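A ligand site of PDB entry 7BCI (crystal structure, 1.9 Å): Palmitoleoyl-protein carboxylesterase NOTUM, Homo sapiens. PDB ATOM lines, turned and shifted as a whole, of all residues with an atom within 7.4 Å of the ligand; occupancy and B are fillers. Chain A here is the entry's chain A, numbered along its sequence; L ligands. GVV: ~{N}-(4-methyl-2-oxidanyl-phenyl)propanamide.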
ATOM      1  N   TRP A  51      -5.221 -11.813  17.128  1.00  0.00           N
ATOM      2  CA  TRP A  51      -4.231 -12.372  18.083  1.00  0.00           C
ATOM      3  C   TRP A  51      -4.976 -12.974  19.286  1.00  0.00           C
ATOM      4  O   TRP A  51      -6.080 -13.515  19.142  1.00  0.00           O
ATOM      5  CB  TRP A  51      -3.176 -11.333  18.416  1.00  0.00           C
ATOM      6  CG  TRP A  51      -2.268 -11.091  17.238  1.00  0.00           C
ATOM      7  CD1 TRP A  51      -2.189  -9.959  16.471  1.00  0.00           C
ATOM      8  CD2 TRP A  51      -1.351 -12.031  16.656  1.00  0.00           C
ATOM      9  NE1 TRP A  51      -1.263 -10.122  15.470  1.00  0.00           N
ATOM     10  CE2 TRP A  51      -0.732 -11.383  15.559  1.00  0.00           C
ATOM     11  CE3 TRP A  51      -0.977 -13.335  16.966  1.00  0.00           C
ATOM     12  CZ2 TRP A  51       0.231 -12.019  14.772  1.00  0.00           C
ATOM     13  CZ3 TRP A  51      -0.016 -13.956  16.187  1.00  0.00           C
ATOM     14  CH2 TRP A  51       0.573 -13.296  15.096  1.00  0.00           C
ATOM     15  N   PHE A 191      -1.375 -22.428   9.705  1.00  0.00           N
ATOM     16  CA  PHE A 191      -0.002 -22.094  10.055  1.00  0.00           C
ATOM     17  C   PHE A 191       0.876 -23.335  10.167  1.00  0.00           C
ATOM     18  O   PHE A 191       0.385 -24.466  10.265  1.00  0.00           O
ATOM     19  CB  PHE A 191       0.056 -21.303  11.382  1.00  0.00           C
ATOM     20  CG  PHE A 191      -0.696 -20.007  11.329  1.00  0.00           C
ATOM     21  CD1 PHE A 191      -1.924 -19.879  11.958  1.00  0.00           C
ATOM     22  CD2 PHE A 191      -0.194 -18.926  10.631  1.00  0.00           C
ATOM     23  CE1 PHE A 191      -2.634 -18.695  11.904  1.00  0.00           C
ATOM     24  CE2 PHE A 191      -0.897 -17.735  10.567  1.00  0.00           C
ATOM     25  CZ  PHE A 191      -2.117 -17.620  11.212  1.00  0.00           C
ATOM     26  N   LEU A 192       2.183 -23.104  10.146  1.00  0.00           N
ATOM     27  CA  LEU A 192       3.189 -24.155  10.229  1.00  0.00           C
ATOM     28  C   LEU A 192       4.021 -23.953  11.478  1.00  0.00           C
ATOM     29  O   LEU A 192       4.485 -22.841  11.749  1.00  0.00           O
ATOM     30  CB  LEU A 192       4.094 -24.150   8.992  1.00  0.00           C
ATOM     31  CG  LEU A 192       3.431 -24.336   7.618  1.00  0.00           C
ATOM     32  CD1 LEU A 192       4.499 -24.454   6.529  1.00  0.00           C
ATOM     33  CD2 LEU A 192       2.507 -25.546   7.600  1.00  0.00           C
ATOM     34  N   ASP A 193       4.214 -25.029  12.240  1.00  0.00           N
ATOM     35  CA  ASP A 193       5.117 -25.012  13.387  1.00  0.00           C
ATOM     36  C   ASP A 193       6.550 -25.331  12.940  1.00  0.00           C
ATOM     37  O   ASP A 193       7.151 -26.342  13.291  1.00  0.00           O
ATOM     38  CB  ASP A 193       4.614 -25.970  14.461  1.00  0.00           C
ATOM     39  CG  ASP A 193       4.319 -27.354  13.912  1.00  0.00           C
ATOM     40  OD1 ASP A 193       4.082 -27.472  12.698  1.00  0.00           O
ATOM     41  OD2 ASP A 193       4.283 -28.321  14.702  1.00  0.00           O
ATOM     42  N   ASN A 194       7.092 -24.415  12.141  1.00  0.00           N
ATOM     43  CA  ASN A 194       8.395 -24.576  11.523  1.00  0.00           C
ATOM     44  C   ASN A 194       9.490 -23.948  12.376  1.00  0.00           C
ATOM     45  O   ASN A 194       9.234 -23.220  13.344  1.00  0.00           O
ATOM     46  CB  ASN A 194       8.387 -23.966  10.120  1.00  0.00           C
ATOM     47  CG  ASN A 194       8.142 -22.471  10.143  1.00  0.00           C
ATOM     48  OD1 ASN A 194       7.676 -21.914  11.144  1.00  0.00           O
ATOM     49  ND2 ASN A 194       8.473 -21.793   9.043  1.00  0.00           N
ATOM     50  N   LYS A 195      10.729 -24.225  11.997  1.00  0.00           N
ATOM     51  CA  LYS A 195      11.880 -23.599  12.649  1.00  0.00           C
ATOM     52  C   LYS A 195      11.935 -22.115  12.304  1.00  0.00           C
ATOM     53  O   LYS A 195      11.747 -21.729  11.151  1.00  0.00           O
ATOM     54  CB  LYS A 195      13.171 -24.286  12.219  1.00  0.00           C
ATOM     55  N   GLN A 196      12.184 -21.283  13.317  1.00  0.00           N
ATOM     56  CA  GLN A 196      12.231 -19.854  13.105  1.00  0.00           C
ATOM     57  C   GLN A 196      13.527 -19.443  12.407  1.00  0.00           C
ATOM     58  O   GLN A 196      14.532 -20.160  12.434  1.00  0.00           O
ATOM     59  CB  GLN A 196      12.109 -19.111  14.435  1.00  0.00           C
ATOM     60  CG  GLN A 196      10.756 -19.281  15.126  1.00  0.00           C
ATOM     61  CD  GLN A 196      10.741 -18.695  16.528  1.00  0.00           C
ATOM     62  OE1 GLN A 196      11.466 -19.154  17.414  1.00  0.00           O
ATOM     63  NE2 GLN A 196       9.908 -17.683  16.744  1.00  0.00           N
ATOM     64  N   PRO A 210       6.664 -20.377  20.396  1.00  0.00           N
ATOM     65  CA  PRO A 210       5.268 -20.062  20.069  1.00  0.00           C
ATOM     66  C   PRO A 210       4.335 -21.231  20.383  1.00  0.00           C
ATOM     67  O   PRO A 210       3.188 -21.009  20.771  1.00  0.00           O
ATOM     68  CB  PRO A 210       5.321 -19.789  18.563  1.00  0.00           C
ATOM     69  CG  PRO A 210       6.695 -19.248  18.345  1.00  0.00           C
ATOM     70  CD  PRO A 210       7.585 -19.991  19.313  1.00  0.00           C
ATOM     71  N   THR A 211       4.828 -22.462  20.217  1.00  0.00           N
ATOM     72  CA  THR A 211       4.058 -23.623  20.643  1.00  0.00           C
ATOM     73  C   THR A 211       3.822 -23.617  22.149  1.00  0.00           C
ATOM     74  O   THR A 211       2.784 -24.103  22.603  1.00  0.00           O
ATOM     75  CB  THR A 211       4.760 -24.929  20.221  1.00  0.00           C
ATOM     76  OG1 THR A 211       6.054 -25.009  20.830  1.00  0.00           O
ATOM     77  CG2 THR A 211       4.879 -25.025  18.717  1.00  0.00           C
ATOM     78  N   GLU A 212       4.753 -23.062  22.916  1.00  0.00           N
ATOM     79  CA  GLU A 212       4.559 -22.963  24.354  1.00  0.00           C
ATOM     80  C   GLU A 212       3.439 -21.996  24.704  1.00  0.00           C
ATOM     81  O   GLU A 212       2.697 -22.216  25.665  1.00  0.00           O
ATOM     82  CB  GLU A 212       5.861 -22.545  25.038  1.00  0.00           C
ATOM     83  N   ILE A 214       0.663 -21.373  23.025  1.00  0.00           N
ATOM     84  CA  ILE A 214      -0.634 -22.003  22.832  1.00  0.00           C
ATOM     85  C   ILE A 214      -0.902 -23.026  23.938  1.00  0.00           C
ATOM     86  O   ILE A 214      -2.005 -23.082  24.502  1.00  0.00           O
ATOM     87  CB  ILE A 214      -0.720 -22.649  21.442  1.00  0.00           C
ATOM     88  CG1 ILE A 214      -0.620 -21.585  20.335  1.00  0.00           C
ATOM     89  CG2 ILE A 214      -2.016 -23.426  21.295  1.00  0.00           C
ATOM     90  CD1 ILE A 214      -1.730 -20.563  20.384  1.00  0.00           C
ATOM     91  N   TRP A 239      -2.467 -28.714  21.838  1.00  0.00           N
ATOM     92  CA  TRP A 239      -1.972 -27.593  21.046  1.00  0.00           C
ATOM     93  C   TRP A 239      -1.743 -27.975  19.586  1.00  0.00           C
ATOM     94  O   TRP A 239      -1.783 -27.109  18.704  1.00  0.00           O
ATOM     95  CB  TRP A 239      -0.676 -27.029  21.644  1.00  0.00           C
ATOM     96  CG  TRP A 239       0.483 -27.989  21.616  1.00  0.00           C
ATOM     97  CD1 TRP A 239       0.849 -28.840  22.618  1.00  0.00           C
ATOM     98  CD2 TRP A 239       1.398 -28.214  20.542  1.00  0.00           C
ATOM     99  NE1 TRP A 239       1.963 -29.560  22.241  1.00  0.00           N
ATOM    100  CE2 TRP A 239       2.306 -29.204  20.967  1.00  0.00           C
ATOM    101  CE3 TRP A 239       1.555 -27.661  19.262  1.00  0.00           C
ATOM    102  CZ2 TRP A 239       3.355 -29.657  20.167  1.00  0.00           C
ATOM    103  CZ3 TRP A 239       2.590 -28.125  18.466  1.00  0.00           C
ATOM    104  CH2 TRP A 239       3.467 -29.104  18.914  1.00  0.00           C
ATOM    105  N   PHE A 243      -3.050 -26.372  14.603  1.00  0.00           N
ATOM    106  CA  PHE A 243      -2.325 -26.289  13.351  1.00  0.00           C
ATOM    107  C   PHE A 243      -3.104 -27.000  12.249  1.00  0.00           C
ATOM    108  O   PHE A 243      -3.357 -28.199  12.331  1.00  0.00           O
ATOM    109  CB  PHE A 243      -0.921 -26.883  13.497  1.00  0.00           C
ATOM    110  CG  PHE A 243      -0.028 -26.043  14.334  1.00  0.00           C
ATOM    111  CD1 PHE A 243       0.009 -26.173  15.711  1.00  0.00           C
ATOM    112  CD2 PHE A 243       0.775 -25.081  13.744  1.00  0.00           C
ATOM    113  CE1 PHE A 243       0.824 -25.367  16.477  1.00  0.00           C
ATOM    114  CE2 PHE A 243       1.597 -24.269  14.500  1.00  0.00           C
ATOM    115  CZ  PHE A 243       1.630 -24.418  15.862  1.00  0.00           C
ATOM    116  N   ASP A 263       2.606 -15.873   4.257  1.00  0.00           N
ATOM    117  CA  ASP A 263       1.738 -15.132   5.160  1.00  0.00           C
ATOM    118  C   ASP A 263       2.553 -14.226   6.090  1.00  0.00           C
ATOM    119  O   ASP A 263       3.578 -14.639   6.633  1.00  0.00           O
ATOM    120  CB  ASP A 263       0.896 -16.110   5.979  1.00  0.00           C
ATOM    121  CG  ASP A 263      -0.101 -15.421   6.869  1.00  0.00           C
ATOM    122  OD1 ASP A 263      -1.222 -15.134   6.405  1.00  0.00           O
ATOM    123  OD2 ASP A 263       0.229 -15.166   8.046  1.00  0.00           O
ATOM    124  N   ALA A 265       1.689 -12.959   9.081  1.00  0.00           N
ATOM    125  CA  ALA A 265       1.675 -13.389  10.482  1.00  0.00           C
ATOM    126  C   ALA A 265       2.641 -14.537  10.708  1.00  0.00           C
ATOM    127  O   ALA A 265       3.372 -14.558  11.708  1.00  0.00           O
ATOM    128  CB  ALA A 265       0.256 -13.769  10.898  1.00  0.00           C
ATOM    129  N   GLN A 266       2.660 -15.504   9.782  1.00  0.00           N
ATOM    130  CA  GLN A 266       3.617 -16.610   9.856  1.00  0.00           C
ATOM    131  C   GLN A 266       5.068 -16.103   9.858  1.00  0.00           C
ATOM    132  O   GLN A 266       5.874 -16.504  10.691  1.00  0.00           O
ATOM    133  CB  GLN A 266       3.392 -17.570   8.687  1.00  0.00           C
ATOM    134  CG  GLN A 266       4.433 -18.679   8.531  1.00  0.00           C
ATOM    135  CD  GLN A 266       4.112 -19.902   9.358  1.00  0.00           C
ATOM    136  OE1 GLN A 266       2.999 -20.426   9.333  1.00  0.00           O
ATOM    137  NE2 GLN A 266       5.113 -20.387  10.090  1.00  0.00           N
ATOM    138  N   LEU A 267       5.390 -15.198   8.927  1.00  0.00           N
ATOM    139  CA  LEU A 267       6.755 -14.703   8.837  1.00  0.00           C
ATOM    140  C   LEU A 267       7.134 -13.862  10.055  1.00  0.00           C
ATOM    141  O   LEU A 267       8.281 -13.888  10.513  1.00  0.00           O
ATOM    142  CB  LEU A 267       6.926 -13.905   7.542  1.00  0.00           C
ATOM    143  CG  LEU A 267       7.037 -14.761   6.278  1.00  0.00           C
ATOM    144  CD1 LEU A 267       6.954 -13.894   5.028  1.00  0.00           C
ATOM    145  CD2 LEU A 267       8.335 -15.539   6.292  1.00  0.00           C
ATOM    146  N   THR A 268       6.164 -13.110  10.594  1.00  0.00           N
ATOM    147  CA  THR A 268       6.428 -12.311  11.795  1.00  0.00           C
ATOM    148  C   THR A 268       6.831 -13.194  12.964  1.00  0.00           C
ATOM    149  O   THR A 268       7.814 -12.922  13.663  1.00  0.00           O
ATOM    150  CB  THR A 268       5.189 -11.488  12.151  1.00  0.00           C
ATOM    151  OG1 THR A 268       5.012 -10.443  11.182  1.00  0.00           O
ATOM    152  CG2 THR A 268       5.336 -10.875  13.535  1.00  0.00           C
ATOM    153  N   VAL A 269       6.068 -14.261  13.204  1.00  0.00           N
ATOM    154  CA  VAL A 269       6.409 -15.175  14.285  1.00  0.00           C
ATOM    155  C   VAL A 269       7.743 -15.870  14.001  1.00  0.00           C
ATOM    156  O   VAL A 269       8.491 -16.191  14.930  1.00  0.00           O
ATOM    157  CB  VAL A 269       5.261 -16.176  14.500  1.00  0.00           C
ATOM    158  CG1 VAL A 269       5.644 -17.230  15.523  1.00  0.00           C
ATOM    159  CG2 VAL A 269       4.005 -15.437  14.955  1.00  0.00           C
ATOM    160  N   ASP A 270       8.062 -16.085  12.729  1.00  0.00           N
ATOM    161  CA  ASP A 270       9.345 -16.656  12.325  1.00  0.00           C
ATOM    162  C   ASP A 270      10.495 -15.658  12.442  1.00  0.00           C
ATOM    163  O   ASP A 270      11.642 -16.019  12.112  1.00  0.00           O
ATOM    164  CB  ASP A 270       9.261 -17.179  10.886  1.00  0.00           C
ATOM    165  CG  ASP A 270       8.550 -18.514  10.792  1.00  0.00           C
ATOM    166  OD1 ASP A 270       8.535 -19.279  11.783  1.00  0.00           O
ATOM    167  OD2 ASP A 270       7.975 -18.804   9.717  1.00  0.00           O
ATOM    168  N   ASN A 271      10.229 -14.424  12.891  1.00  0.00           N
ATOM    169  CA  ASN A 271      11.236 -13.377  13.037  1.00  0.00           C
ATOM    170  C   ASN A 271      11.906 -13.034  11.705  1.00  0.00           C
ATOM    171  O   ASN A 271      13.118 -12.826  11.636  1.00  0.00           O
ATOM    172  CB  ASN A 271      12.281 -13.735  14.101  1.00  0.00           C
ATOM    173  CG  ASN A 271      11.685 -13.884  15.484  1.00  0.00           C
ATOM    174  OD1 ASN A 271      10.928 -13.023  15.935  1.00  0.00           O
ATOM    175  ND2 ASN A 271      12.032 -14.960  16.177  1.00  0.00           N
ATOM    176  N   TYR A 286      15.347 -19.799   3.118  1.00  0.00           N
ATOM    177  CA  TYR A 286      14.318 -19.914   4.150  1.00  0.00           C
ATOM    178  C   TYR A 286      12.927 -19.644   3.573  1.00  0.00           C
ATOM    179  O   TYR A 286      12.003 -20.452   3.728  1.00  0.00           O
ATOM    180  CB  TYR A 286      14.592 -18.932   5.288  1.00  0.00           C
ATOM    181  CG  TYR A 286      13.690 -19.118   6.485  1.00  0.00           C
ATOM    182  CD1 TYR A 286      14.001 -20.037   7.476  1.00  0.00           C
ATOM    183  CD2 TYR A 286      12.482 -18.434   6.580  1.00  0.00           C
ATOM    184  CE1 TYR A 286      13.170 -20.230   8.564  1.00  0.00           C
ATOM    185  CE2 TYR A 286      11.638 -18.628   7.667  1.00  0.00           C
ATOM    186  CZ  TYR A 286      11.989 -19.524   8.651  1.00  0.00           C
ATOM    187  OH  TYR A 286      11.151 -19.712   9.728  1.00  0.00           O
HETATM  188  N1  GVV L   1       7.460 -22.459  15.318  1.00  0.00           N
HETATM  189  C4  GVV L   1       6.300 -21.679  14.885  1.00  0.00           C
HETATM  190  C5  GVV L   1       6.502 -20.711  13.922  1.00  0.00           C
HETATM  191  C6  GVV L   1       5.431 -19.940  13.457  1.00  0.00           C
HETATM  192  C7  GVV L   1       4.163 -20.143  13.967  1.00  0.00           C
HETATM  193  C8  GVV L   1       3.961 -21.111  14.930  1.00  0.00           C
HETATM  194  C10 GVV L   1       2.992 -19.303  13.477  1.00  0.00           C
HETATM  195  C1  GVV L   1       9.050 -25.086  16.122  1.00  0.00           C
HETATM  196  C2  GVV L   1       8.899 -23.820  16.970  1.00  0.00           C
HETATM  197  C3  GVV L   1       7.633 -23.041  16.638  1.00  0.00           C
HETATM  198  O1  GVV L   1       6.801 -22.917  17.469  1.00  0.00           O
HETATM  199  C9  GVV L   1       5.019 -21.883  15.394  1.00  0.00           C
HETATM  200  O2  GVV L   1       4.758 -22.851  16.367  1.00  0.00           O
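The side-chain amide oxygen of Asn 194 lies close to the side-chain carboxylate of Asp 270, 2.8 Å away. OD1 of Asn 194 lies close to O of Leu 192 (3.4 Å). The side-chain hydroxyl (OH) of Tyr 286 is in hydrogen-bond range of the side-chain amide nitrogen (ND2) of Asn 194 (3.5 Å). NE2 of Gln 266 is in hydrogen-bond range of OD2 of Asp 270 (3.3 Å). The side-chain carboxylate (OD2) of Asp 270 sits close to the side-chain hydroxyl (OH) of Tyr 286 (3.3 Å). N of Leu 192 sits at hydrogen-bond distance from OE1 of Gln 266 (2.9 Å). N of Gln 266 sits at hydrogen-bond distance from OD2 of Asp 263 (3.0 Å). The backbone carbonyl oxygen (O) of Val 269 sits at hydrogen-bond distance from the side-chain amide nitrogen (NE2) of Gln 196 (2.7 Å).
Residues that only touch the ligand: Asp 270 (3.3 Å), Gln 266 (3.4 Å), Val 269 (3.4 Å), Leu 192 (3.5 Å), Phe 243 (3.5 Å), Pro 210 (3.5 Å) and Asp 193 (3.6 Å). Within 4 Å of the ligand: Leu 192, Asp 193, Asn 194, Pro 210, Thr 211, Phe 243, Gln 266, Val 269 and Asp 270. The nearest printed residue that does not touch the ligand is Phe 191 (4.1 Å).
N1 of the ligand is in hydrogen-bond range of O of Asn 194 (2.8 Å). An oxygen (O1) of the ligand sits close to the backbone NH of Thr 211.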
